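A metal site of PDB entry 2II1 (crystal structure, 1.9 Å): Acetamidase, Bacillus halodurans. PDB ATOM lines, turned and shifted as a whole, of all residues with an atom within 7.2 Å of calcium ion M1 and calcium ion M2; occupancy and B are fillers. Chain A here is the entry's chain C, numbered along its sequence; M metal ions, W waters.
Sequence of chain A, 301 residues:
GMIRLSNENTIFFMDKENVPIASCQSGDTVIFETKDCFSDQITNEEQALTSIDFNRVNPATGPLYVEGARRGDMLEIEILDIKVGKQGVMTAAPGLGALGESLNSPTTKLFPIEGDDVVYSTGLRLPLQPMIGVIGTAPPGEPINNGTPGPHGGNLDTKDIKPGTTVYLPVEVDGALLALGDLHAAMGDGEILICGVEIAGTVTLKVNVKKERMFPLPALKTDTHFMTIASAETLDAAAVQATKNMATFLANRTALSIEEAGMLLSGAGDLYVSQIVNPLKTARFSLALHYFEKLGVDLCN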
ATOM      1  N   ASP A  36     -26.667  -5.624  -2.284  1.00  0.00           N
ATOM      2  CA  ASP A  36     -26.776  -5.329  -3.720  1.00  0.00           C
ATOM      3  C   ASP A  36     -27.939  -4.333  -3.902  1.00  0.00           C
ATOM      4  O   ASP A  36     -28.686  -4.061  -2.941  1.00  0.00           O
ATOM      5  CB  ASP A  36     -26.888  -6.594  -4.614  1.00  0.00           C
ATOM      6  CG  ASP A  36     -28.279  -7.251  -4.603  1.00  0.00           C
ATOM      7  OD1 ASP A  36     -29.267  -6.583  -4.221  1.00  0.00           O
ATOM      8  OD2 ASP A  36     -28.384  -8.427  -4.995  1.00  0.00           O
ATOM      9  N   CYS A  37     -28.089  -3.779  -5.105  1.00  0.00           N
ATOM     10  CA  CYS A  37     -29.000  -2.641  -5.243  1.00  0.00           C
ATOM     11  C   CYS A  37     -30.467  -3.028  -5.243  1.00  0.00           C
ATOM     12  O   CYS A  37     -31.333  -2.177  -5.316  1.00  0.00           O
ATOM     13  CB  CYS A  37     -28.610  -1.743  -6.413  1.00  0.00           C
ATOM     14  SG  CYS A  37     -29.059  -2.293  -8.005  1.00  0.00           S
ATOM     15  N   PHE A  38     -30.745  -4.329  -5.149  1.00  0.00           N
ATOM     16  CA  PHE A  38     -32.103  -4.809  -4.888  1.00  0.00           C
ATOM     17  C   PHE A  38     -32.318  -5.057  -3.389  1.00  0.00           C
ATOM     18  O   PHE A  38     -33.330  -5.631  -2.997  1.00  0.00           O
ATOM     19  CB  PHE A  38     -32.393  -6.095  -5.689  1.00  0.00           C
ATOM     20  CG  PHE A  38     -32.243  -5.926  -7.197  1.00  0.00           C
ATOM     21  CD1 PHE A  38     -33.047  -5.010  -7.888  1.00  0.00           C
ATOM     22  CD2 PHE A  38     -31.315  -6.684  -7.911  1.00  0.00           C
ATOM     23  CE1 PHE A  38     -32.913  -4.843  -9.271  1.00  0.00           C
ATOM     24  CE2 PHE A  38     -31.199  -6.543  -9.306  1.00  0.00           C
ATOM     25  CZ  PHE A  38     -31.988  -5.625  -9.980  1.00  0.00           C
ATOM     26  N   ASN A  58     -31.549   0.389  -4.285  1.00  0.00           N
ATOM     27  CA  ASN A  58     -30.402   1.297  -4.169  1.00  0.00           C
ATOM     28  C   ASN A  58     -30.040   1.691  -2.749  1.00  0.00           C
ATOM     29  O   ASN A  58     -29.976   2.892  -2.445  1.00  0.00           O
ATOM     30  CB  ASN A  58     -30.569   2.561  -5.009  1.00  0.00           C
ATOM     31  CG  ASN A  58     -30.445   2.305  -6.464  1.00  0.00           C
ATOM     32  OD1 ASN A  58     -31.239   2.811  -7.271  1.00  0.00           O
ATOM     33  ND2 ASN A  58     -29.451   1.515  -6.826  1.00  0.00           N
ATOM     34  N   MET A 131     -16.557  -2.767  -9.186  1.00  0.00           N
ATOM     35  CA  MET A 131     -16.727  -1.303  -9.199  1.00  0.00           C
ATOM     36  C   MET A 131     -17.833  -0.888  -8.234  1.00  0.00           C
ATOM     37  O   MET A 131     -18.624  -1.711  -7.767  1.00  0.00           O
ATOM     38  CB  MET A 131     -17.050  -0.784 -10.607  1.00  0.00           C
ATOM     39  CG  MET A 131     -18.251  -1.508 -11.247  1.00  0.00           C
ATOM     40  SD  MET A 131     -19.164  -0.601 -12.700  1.00  0.00           S
ATOM     41  CE  MET A 131     -19.947   1.000 -11.704  1.00  0.00           C
ATOM     42  N   GLY A 133     -21.107   1.527  -7.880  1.00  0.00           N
ATOM     43  CA  GLY A 133     -22.110   2.206  -8.710  1.00  0.00           C
ATOM     44  C   GLY A 133     -22.684   3.475  -8.135  1.00  0.00           C
ATOM     45  O   GLY A 133     -22.847   4.486  -8.847  1.00  0.00           O
ATOM     46  N   VAL A 134     -22.970   3.439  -6.834  1.00  0.00           N
ATOM     47  CA  VAL A 134     -23.499   4.581  -6.102  1.00  0.00           C
ATOM     48  C   VAL A 134     -22.467   5.046  -5.055  1.00  0.00           C
ATOM     49  O   VAL A 134     -22.014   4.268  -4.208  1.00  0.00           O
ATOM     50  CB  VAL A 134     -24.869   4.243  -5.427  1.00  0.00           C
ATOM     51  CG1 VAL A 134     -25.273   5.359  -4.411  1.00  0.00           C
ATOM     52  CG2 VAL A 134     -25.957   3.971  -6.494  1.00  0.00           C
ATOM     53  N   ASN A 146     -31.081   7.992  -3.981  1.00  0.00           N
ATOM     54  CA  ASN A 146     -29.770   7.432  -4.369  1.00  0.00           C
ATOM     55  C   ASN A 146     -29.642   7.087  -5.856  1.00  0.00           C
ATOM     56  O   ASN A 146     -28.542   7.055  -6.406  1.00  0.00           O
ATOM     57  CB  ASN A 146     -29.466   6.157  -3.583  1.00  0.00           C
ATOM     58  CG  ASN A 146     -29.155   6.420  -2.124  1.00  0.00           C
ATOM     59  OD1 ASN A 146     -29.075   7.573  -1.685  1.00  0.00           O
ATOM     60  ND2 ASN A 146     -29.001   5.323  -1.357  1.00  0.00           N
ATOM     61  N   GLY A 147     -30.770   6.800  -6.510  1.00  0.00           N
ATOM     62  CA  GLY A 147     -30.782   6.389  -7.907  1.00  0.00           C
ATOM     63  C   GLY A 147     -30.624   7.491  -8.927  1.00  0.00           C
ATOM     64  O   GLY A 147     -30.591   7.204 -10.113  1.00  0.00           O
ATOM     65  N   GLY A 154     -23.970  10.232  -6.132  1.00  0.00           N
ATOM     66  CA  GLY A 154     -25.122   9.365  -6.348  1.00  0.00           C
ATOM     67  C   GLY A 154     -24.902   8.192  -7.294  1.00  0.00           C
ATOM     68  O   GLY A 154     -23.845   7.561  -7.354  1.00  0.00           O
ATOM     69  N   ASN A 155     -25.920   7.936  -8.088  1.00  0.00           N
ATOM     70  CA  ASN A 155     -26.001   6.816  -9.021  1.00  0.00           C
ATOM     71  C   ASN A 155     -25.198   7.112 -10.304  1.00  0.00           C
ATOM     72  O   ASN A 155     -25.774   7.229 -11.378  1.00  0.00           O
ATOM     73  CB  ASN A 155     -27.483   6.608  -9.338  1.00  0.00           C
ATOM     74  CG  ASN A 155     -27.805   5.268  -9.909  1.00  0.00           C
ATOM     75  OD1 ASN A 155     -26.955   4.394  -9.972  1.00  0.00           O
ATOM     76  ND2 ASN A 155     -29.096   5.070 -10.330  1.00  0.00           N
ATOM     77  N   LEU A 156     -23.861   7.188 -10.192  1.00  0.00           N
ATOM     78  CA  LEU A 156     -22.929   7.492 -11.325  1.00  0.00           C
ATOM     79  C   LEU A 156     -22.639   6.348 -12.312  1.00  0.00           C
ATOM     80  O   LEU A 156     -22.225   6.606 -13.447  1.00  0.00           O
ATOM     81  CB  LEU A 156     -21.580   7.983 -10.793  1.00  0.00           C
ATOM     82  CG  LEU A 156     -21.606   9.206  -9.883  1.00  0.00           C
ATOM     83  CD1 LEU A 156     -20.202   9.569  -9.395  1.00  0.00           C
ATOM     84  CD2 LEU A 156     -22.275  10.391 -10.602  1.00  0.00           C
ATOM     85  N   ASP A 157     -22.810   5.096 -11.885  1.00  0.00           N
ATOM     86  CA  ASP A 157     -22.472   3.885 -12.684  1.00  0.00           C
ATOM     87  C   ASP A 157     -21.308   4.074 -13.666  1.00  0.00           C
ATOM     88  O   ASP A 157     -21.440   3.878 -14.872  1.00  0.00           O
ATOM     89  CB  ASP A 157     -23.729   3.340 -13.400  1.00  0.00           C
ATOM     90  CG  ASP A 157     -24.768   2.788 -12.403  1.00  0.00           C
ATOM     91  OD1 ASP A 157     -24.366   2.217 -11.389  1.00  0.00           O
ATOM     92  OD2 ASP A 157     -25.996   2.941 -12.641  1.00  0.00           O
ATOM     93  N   GLY A 181     -22.835   2.389  -2.307  1.00  0.00           N
ATOM     94  CA  GLY A 181     -23.487   1.119  -2.507  1.00  0.00           C
ATOM     95  C   GLY A 181     -23.448   0.695  -3.960  1.00  0.00           C
ATOM     96  O   GLY A 181     -22.623   1.205  -4.756  1.00  0.00           O
ATOM     97  N   ASP A 182     -24.327  -0.243  -4.306  1.00  0.00           N
ATOM     98  CA  ASP A 182     -24.519  -0.684  -5.690  1.00  0.00           C
ATOM     99  C   ASP A 182     -23.225  -1.198  -6.301  1.00  0.00           C
ATOM    100  O   ASP A 182     -22.761  -0.623  -7.286  1.00  0.00           O
ATOM    101  CB  ASP A 182     -25.065   0.498  -6.540  1.00  0.00           C
ATOM    102  CG  ASP A 182     -25.421   0.113  -7.980  1.00  0.00           C
ATOM    103  OD1 ASP A 182     -25.838  -1.053  -8.204  1.00  0.00           O
ATOM    104  OD2 ASP A 182     -25.290   0.952  -8.895  1.00  0.00           O
ATOM    105  N   LEU A 183     -22.616  -2.247  -5.744  1.00  0.00           N
ATOM    106  CA  LEU A 183     -21.402  -2.790  -6.342  1.00  0.00           C
ATOM    107  C   LEU A 183     -21.776  -3.646  -7.533  1.00  0.00           C
ATOM    108  O   LEU A 183     -22.855  -4.205  -7.566  1.00  0.00           O
ATOM    109  CB  LEU A 183     -20.577  -3.625  -5.355  1.00  0.00           C
ATOM    110  CG  LEU A 183     -20.044  -3.034  -4.050  1.00  0.00           C
ATOM    111  CD1 LEU A 183     -19.047  -4.059  -3.399  1.00  0.00           C
ATOM    112  CD2 LEU A 183     -19.419  -1.640  -4.250  1.00  0.00           C
ATOM    113  N   HIS A 184     -20.884  -3.717  -8.519  1.00  0.00           N
ATOM    114  CA  HIS A 184     -21.079  -4.593  -9.673  1.00  0.00           C
ATOM    115  C   HIS A 184     -19.840  -5.457  -9.786  1.00  0.00           C
ATOM    116  O   HIS A 184     -18.753  -4.974  -9.530  1.00  0.00           O
ATOM    117  CB  HIS A 184     -21.251  -3.833 -10.995  1.00  0.00           C
ATOM    118  CG  HIS A 184     -22.400  -2.868 -11.009  1.00  0.00           C
ATOM    119  ND1 HIS A 184     -22.361  -1.686 -11.705  1.00  0.00           N
ATOM    120  CD2 HIS A 184     -23.617  -2.919 -10.415  1.00  0.00           C
ATOM    121  CE1 HIS A 184     -23.491  -1.031 -11.535  1.00  0.00           C
ATOM    122  NE2 HIS A 184     -24.274  -1.760 -10.760  1.00  0.00           N
ATOM    123  N   MET A 187     -19.685  -4.595 -15.513  1.00  0.00           N
ATOM    124  CA  MET A 187     -20.541  -3.668 -16.235  1.00  0.00           C
ATOM    125  C   MET A 187     -19.714  -2.976 -17.332  1.00  0.00           C
ATOM    126  O   MET A 187     -18.565  -2.640 -17.111  1.00  0.00           O
ATOM    127  CB  MET A 187     -21.106  -2.620 -15.273  1.00  0.00           C
ATOM    128  CG  MET A 187     -22.190  -1.771 -15.845  1.00  0.00           C
ATOM    129  SD  MET A 187     -22.256  -0.059 -14.910  1.00  0.00           S
ATOM    130  CE  MET A 187     -20.770   0.833 -15.793  1.00  0.00           C
ATOM    131  N   GLU A 191     -23.945   0.739 -19.484  1.00  0.00           N
ATOM    132  CA  GLU A 191     -24.887  -0.056 -18.676  1.00  0.00           C
ATOM    133  C   GLU A 191     -26.240  -0.237 -19.393  1.00  0.00           C
ATOM    134  O   GLU A 191     -27.315  -0.045 -18.796  1.00  0.00           O
ATOM    135  CB  GLU A 191     -25.094   0.613 -17.345  1.00  0.00           C
ATOM    136  CG  GLU A 191     -25.779  -0.281 -16.283  1.00  0.00           C
ATOM    137  CD  GLU A 191     -25.960   0.460 -14.978  1.00  0.00           C
ATOM    138  OE1 GLU A 191     -26.210   1.687 -15.003  1.00  0.00           O
ATOM    139  OE2 GLU A 191     -25.841  -0.205 -13.930  1.00  0.00           O
ATOM    140  N   ILE A 194     -29.820  -1.805 -18.231  1.00  0.00           N
ATOM    141  CA  ILE A 194     -30.406  -1.204 -16.994  1.00  0.00           C
ATOM    142  C   ILE A 194     -29.468  -1.465 -15.812  1.00  0.00           C
ATOM    143  O   ILE A 194     -29.344  -0.627 -14.909  1.00  0.00           O
ATOM    144  CB  ILE A 194     -31.911  -1.652 -16.657  1.00  0.00           C
ATOM    145  CG1 ILE A 194     -32.500  -0.890 -15.457  1.00  0.00           C
ATOM    146  CG2 ILE A 194     -32.012  -3.155 -16.314  1.00  0.00           C
ATOM    147  CD1 ILE A 194     -32.680   0.645 -15.640  1.00  0.00           C
ATOM    148  N   CYS A 195     -28.765  -2.588 -15.842  1.00  0.00           N
ATOM    149  CA  CYS A 195     -27.935  -3.035 -14.719  1.00  0.00           C
ATOM    150  C   CYS A 195     -26.562  -3.584 -15.139  1.00  0.00           C
ATOM    151  O   CYS A 195     -26.296  -3.820 -16.318  1.00  0.00           O
ATOM    152  CB  CYS A 195     -28.675  -4.110 -13.911  1.00  0.00           C
ATOM    153  SG  CYS A 195     -29.120  -5.535 -14.867  1.00  0.00           S
ATOM    154  N   GLY A 196     -25.672  -3.676 -14.156  1.00  0.00           N
ATOM    155  CA  GLY A 196     -24.471  -4.496 -14.266  1.00  0.00           C
ATOM    156  C   GLY A 196     -24.753  -5.807 -13.599  1.00  0.00           C
ATOM    157  O   GLY A 196     -25.905  -6.118 -13.282  1.00  0.00           O
ATOM    158  N   VAL A 197     -23.719  -6.608 -13.376  1.00  0.00           N
ATOM    159  CA  VAL A 197     -23.883  -7.806 -12.552  1.00  0.00           C
ATOM    160  C   VAL A 197     -23.972  -7.297 -11.113  1.00  0.00           C
ATOM    161  O   VAL A 197     -22.960  -6.999 -10.489  1.00  0.00           O
ATOM    162  CB  VAL A 197     -22.676  -8.796 -12.735  1.00  0.00           C
ATOM    163  CG1 VAL A 197     -22.808  -9.970 -11.830  1.00  0.00           C
ATOM    164  CG2 VAL A 197     -22.581  -9.233 -14.186  1.00  0.00           C
ATOM    165  N   GLU A 198     -25.203  -7.160 -10.613  1.00  0.00           N
ATOM    166  CA  GLU A 198     -25.462  -6.603  -9.281  1.00  0.00           C
ATOM    167  C   GLU A 198     -24.976  -7.576  -8.205  1.00  0.00           C
ATOM    168  O   GLU A 198     -25.226  -8.772  -8.290  1.00  0.00           O
ATOM    169  CB  GLU A 198     -26.957  -6.360  -9.098  1.00  0.00           C
ATOM    170  CG  GLU A 198     -27.597  -5.517 -10.177  1.00  0.00           C
ATOM    171  CD  GLU A 198     -27.103  -4.118 -10.187  1.00  0.00           C
ATOM    172  OE1 GLU A 198     -26.493  -3.710  -9.167  1.00  0.00           O
ATOM    173  OE2 GLU A 198     -27.317  -3.403 -11.227  1.00  0.00           O
ATOM    174  N   ILE A 199     -24.253  -7.070  -7.213  1.00  0.00           N
ATOM    175  CA  ILE A 199     -23.642  -7.927  -6.205  1.00  0.00           C
ATOM    176  C   ILE A 199     -23.419  -7.189  -4.849  1.00  0.00           C
ATOM    177  O   ILE A 199     -23.235  -5.974  -4.802  1.00  0.00           O
ATOM    178  CB  ILE A 199     -22.311  -8.538  -6.787  1.00  0.00           C
ATOM    179  CG1 ILE A 199     -22.005  -9.890  -6.136  1.00  0.00           C
ATOM    180  CG2 ILE A 199     -21.151  -7.546  -6.686  1.00  0.00           C
ATOM    181  CD1 ILE A 199     -21.093 -10.813  -7.004  1.00  0.00           C
ATOM    182  N   GLN A 275     -23.256   5.790 -18.149  1.00  0.00           N
ATOM    183  CA  GLN A 275     -24.495   5.050 -18.194  1.00  0.00           C
ATOM    184  C   GLN A 275     -25.529   5.943 -18.879  1.00  0.00           C
ATOM    185  O   GLN A 275     -25.421   7.163 -18.812  1.00  0.00           O
ATOM    186  CB  GLN A 275     -24.942   4.660 -16.752  1.00  0.00           C
ATOM    187  CG  GLN A 275     -25.074   5.817 -15.767  1.00  0.00           C
ATOM    188  CD  GLN A 275     -26.365   6.606 -15.901  1.00  0.00           C
ATOM    189  OE1 GLN A 275     -27.349   6.126 -16.510  1.00  0.00           O
ATOM    190  NE2 GLN A 275     -26.394   7.809 -15.311  1.00  0.00           N
ATOM    191  N   VAL A 277     -29.083   5.014 -18.564  1.00  0.00           N
ATOM    192  CA  VAL A 277     -30.310   4.308 -18.134  1.00  0.00           C
ATOM    193  C   VAL A 277     -30.938   4.847 -16.846  1.00  0.00           C
ATOM    194  O   VAL A 277     -32.038   4.433 -16.477  1.00  0.00           O
ATOM    195  CB  VAL A 277     -30.039   2.795 -17.929  1.00  0.00           C
ATOM    196  CG1 VAL A 277     -29.828   2.104 -19.270  1.00  0.00           C
ATOM    197  CG2 VAL A 277     -28.847   2.587 -17.037  1.00  0.00           C
ATOM    198  N   ASN A 278     -30.243   5.749 -16.151  1.00  0.00           N
ATOM    199  CA  ASN A 278     -30.704   6.252 -14.858  1.00  0.00           C
ATOM    200  C   ASN A 278     -31.531   7.510 -15.061  1.00  0.00           C
ATOM    201  O   ASN A 278     -31.647   7.985 -16.201  1.00  0.00           O
ATOM    202  CB  ASN A 278     -29.495   6.498 -13.918  1.00  0.00           C
ATOM    203  CG  ASN A 278     -28.744   5.215 -13.598  1.00  0.00           C
ATOM    204  OD1 ASN A 278     -29.295   4.128 -13.656  1.00  0.00           O
ATOM    205  ND2 ASN A 278     -27.476   5.351 -13.282  1.00  0.00           N
HETATM  206 CA    CA M   1     -26.672   1.970 -10.433  1.00  0.00          CA
HETATM  207 CA    CA M   2     -26.329  -1.657 -10.035  1.00  0.00          CA
HETATM  208  O   HOH W   1     -28.642   2.338 -11.701  1.00  0.00           O
HETATM  209  O   HOH W   2     -26.885  -0.298 -11.460  1.00  0.00           O
HETATM  210  O   HOH W   3     -28.520   1.534  -8.831  1.00  0.00           O
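The side-chain amide nitrogen (ND2) of Asn 278 sits at hydrogen-bond distance from the backbone carbonyl oxygen (O) of Asn 155 (3.2 Å).
The side-chain carboxylate of Glu 191 lies close to the side-chain carboxylate of Asp 157 (2.7 Å).
OD1 of Asp 182 lies close to SG of Cys 37.
The side-chain amide nitrogen of Asn 155 sits at hydrogen-bond distance from the backbone carbonyl oxygen of Gly 147 (2.6 Å).
O of Asp 182 is in hydrogen-bond range of N of Gly 133 (2.8 Å).
SD of Met 187 lies within hydrogen-bond range of ND1 of His 184 (3.6 Å).
The backbone carbonyl oxygen (O) of Gly 133 lies within hydrogen-bond range of the backbone NH (N) of Asp 157 (3.1 Å).
The backbone carbonyl oxygen (O) of Met 131 lies within hydrogen-bond range of the backbone NH (N) of His 184 (3.1 Å).
Of the 28 residues printed, 3 come within 4 Å of calcium ion M1.
Calcium ion M2 is bound by the side-chain carboxylate (OD1) of Asp 182 (2.0 Å), water W2 (2.0 Å), a ring nitrogen (NE2) of His 184 (2.2 Å), the side-chain carboxylate (OE1) of Glu 198 (2.2 Å) and the side-chain carboxylate (OE2) of Glu 198 (2.3 Å).
Slightly farther from calcium ion M2 lies the side-chain carboxylate (OD2) of Asp 182 (3.0 Å).
Residues that only touch calcium ion M2: Cys 37 (3.5 Å).
Water W1 lies within hydrogen-bond range of the side-chain amide oxygen (OD1) of Asn 278 and the side-chain amide nitrogen (ND2) of Asn 155.
Calcium ion M1 is bound by OD2 of Asp 182 (2.3 Å), water W1 (2.4 Å), OD1 of Asn 155 (2.5 Å), water W3 (2.5 Å), water W2 (2.5 Å), OD2 of Asp 157 (2.5 Å) and OD1 of Asp 157 (2.5 Å).
Calcium ion M1 has seven donor atoms within binding distance.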
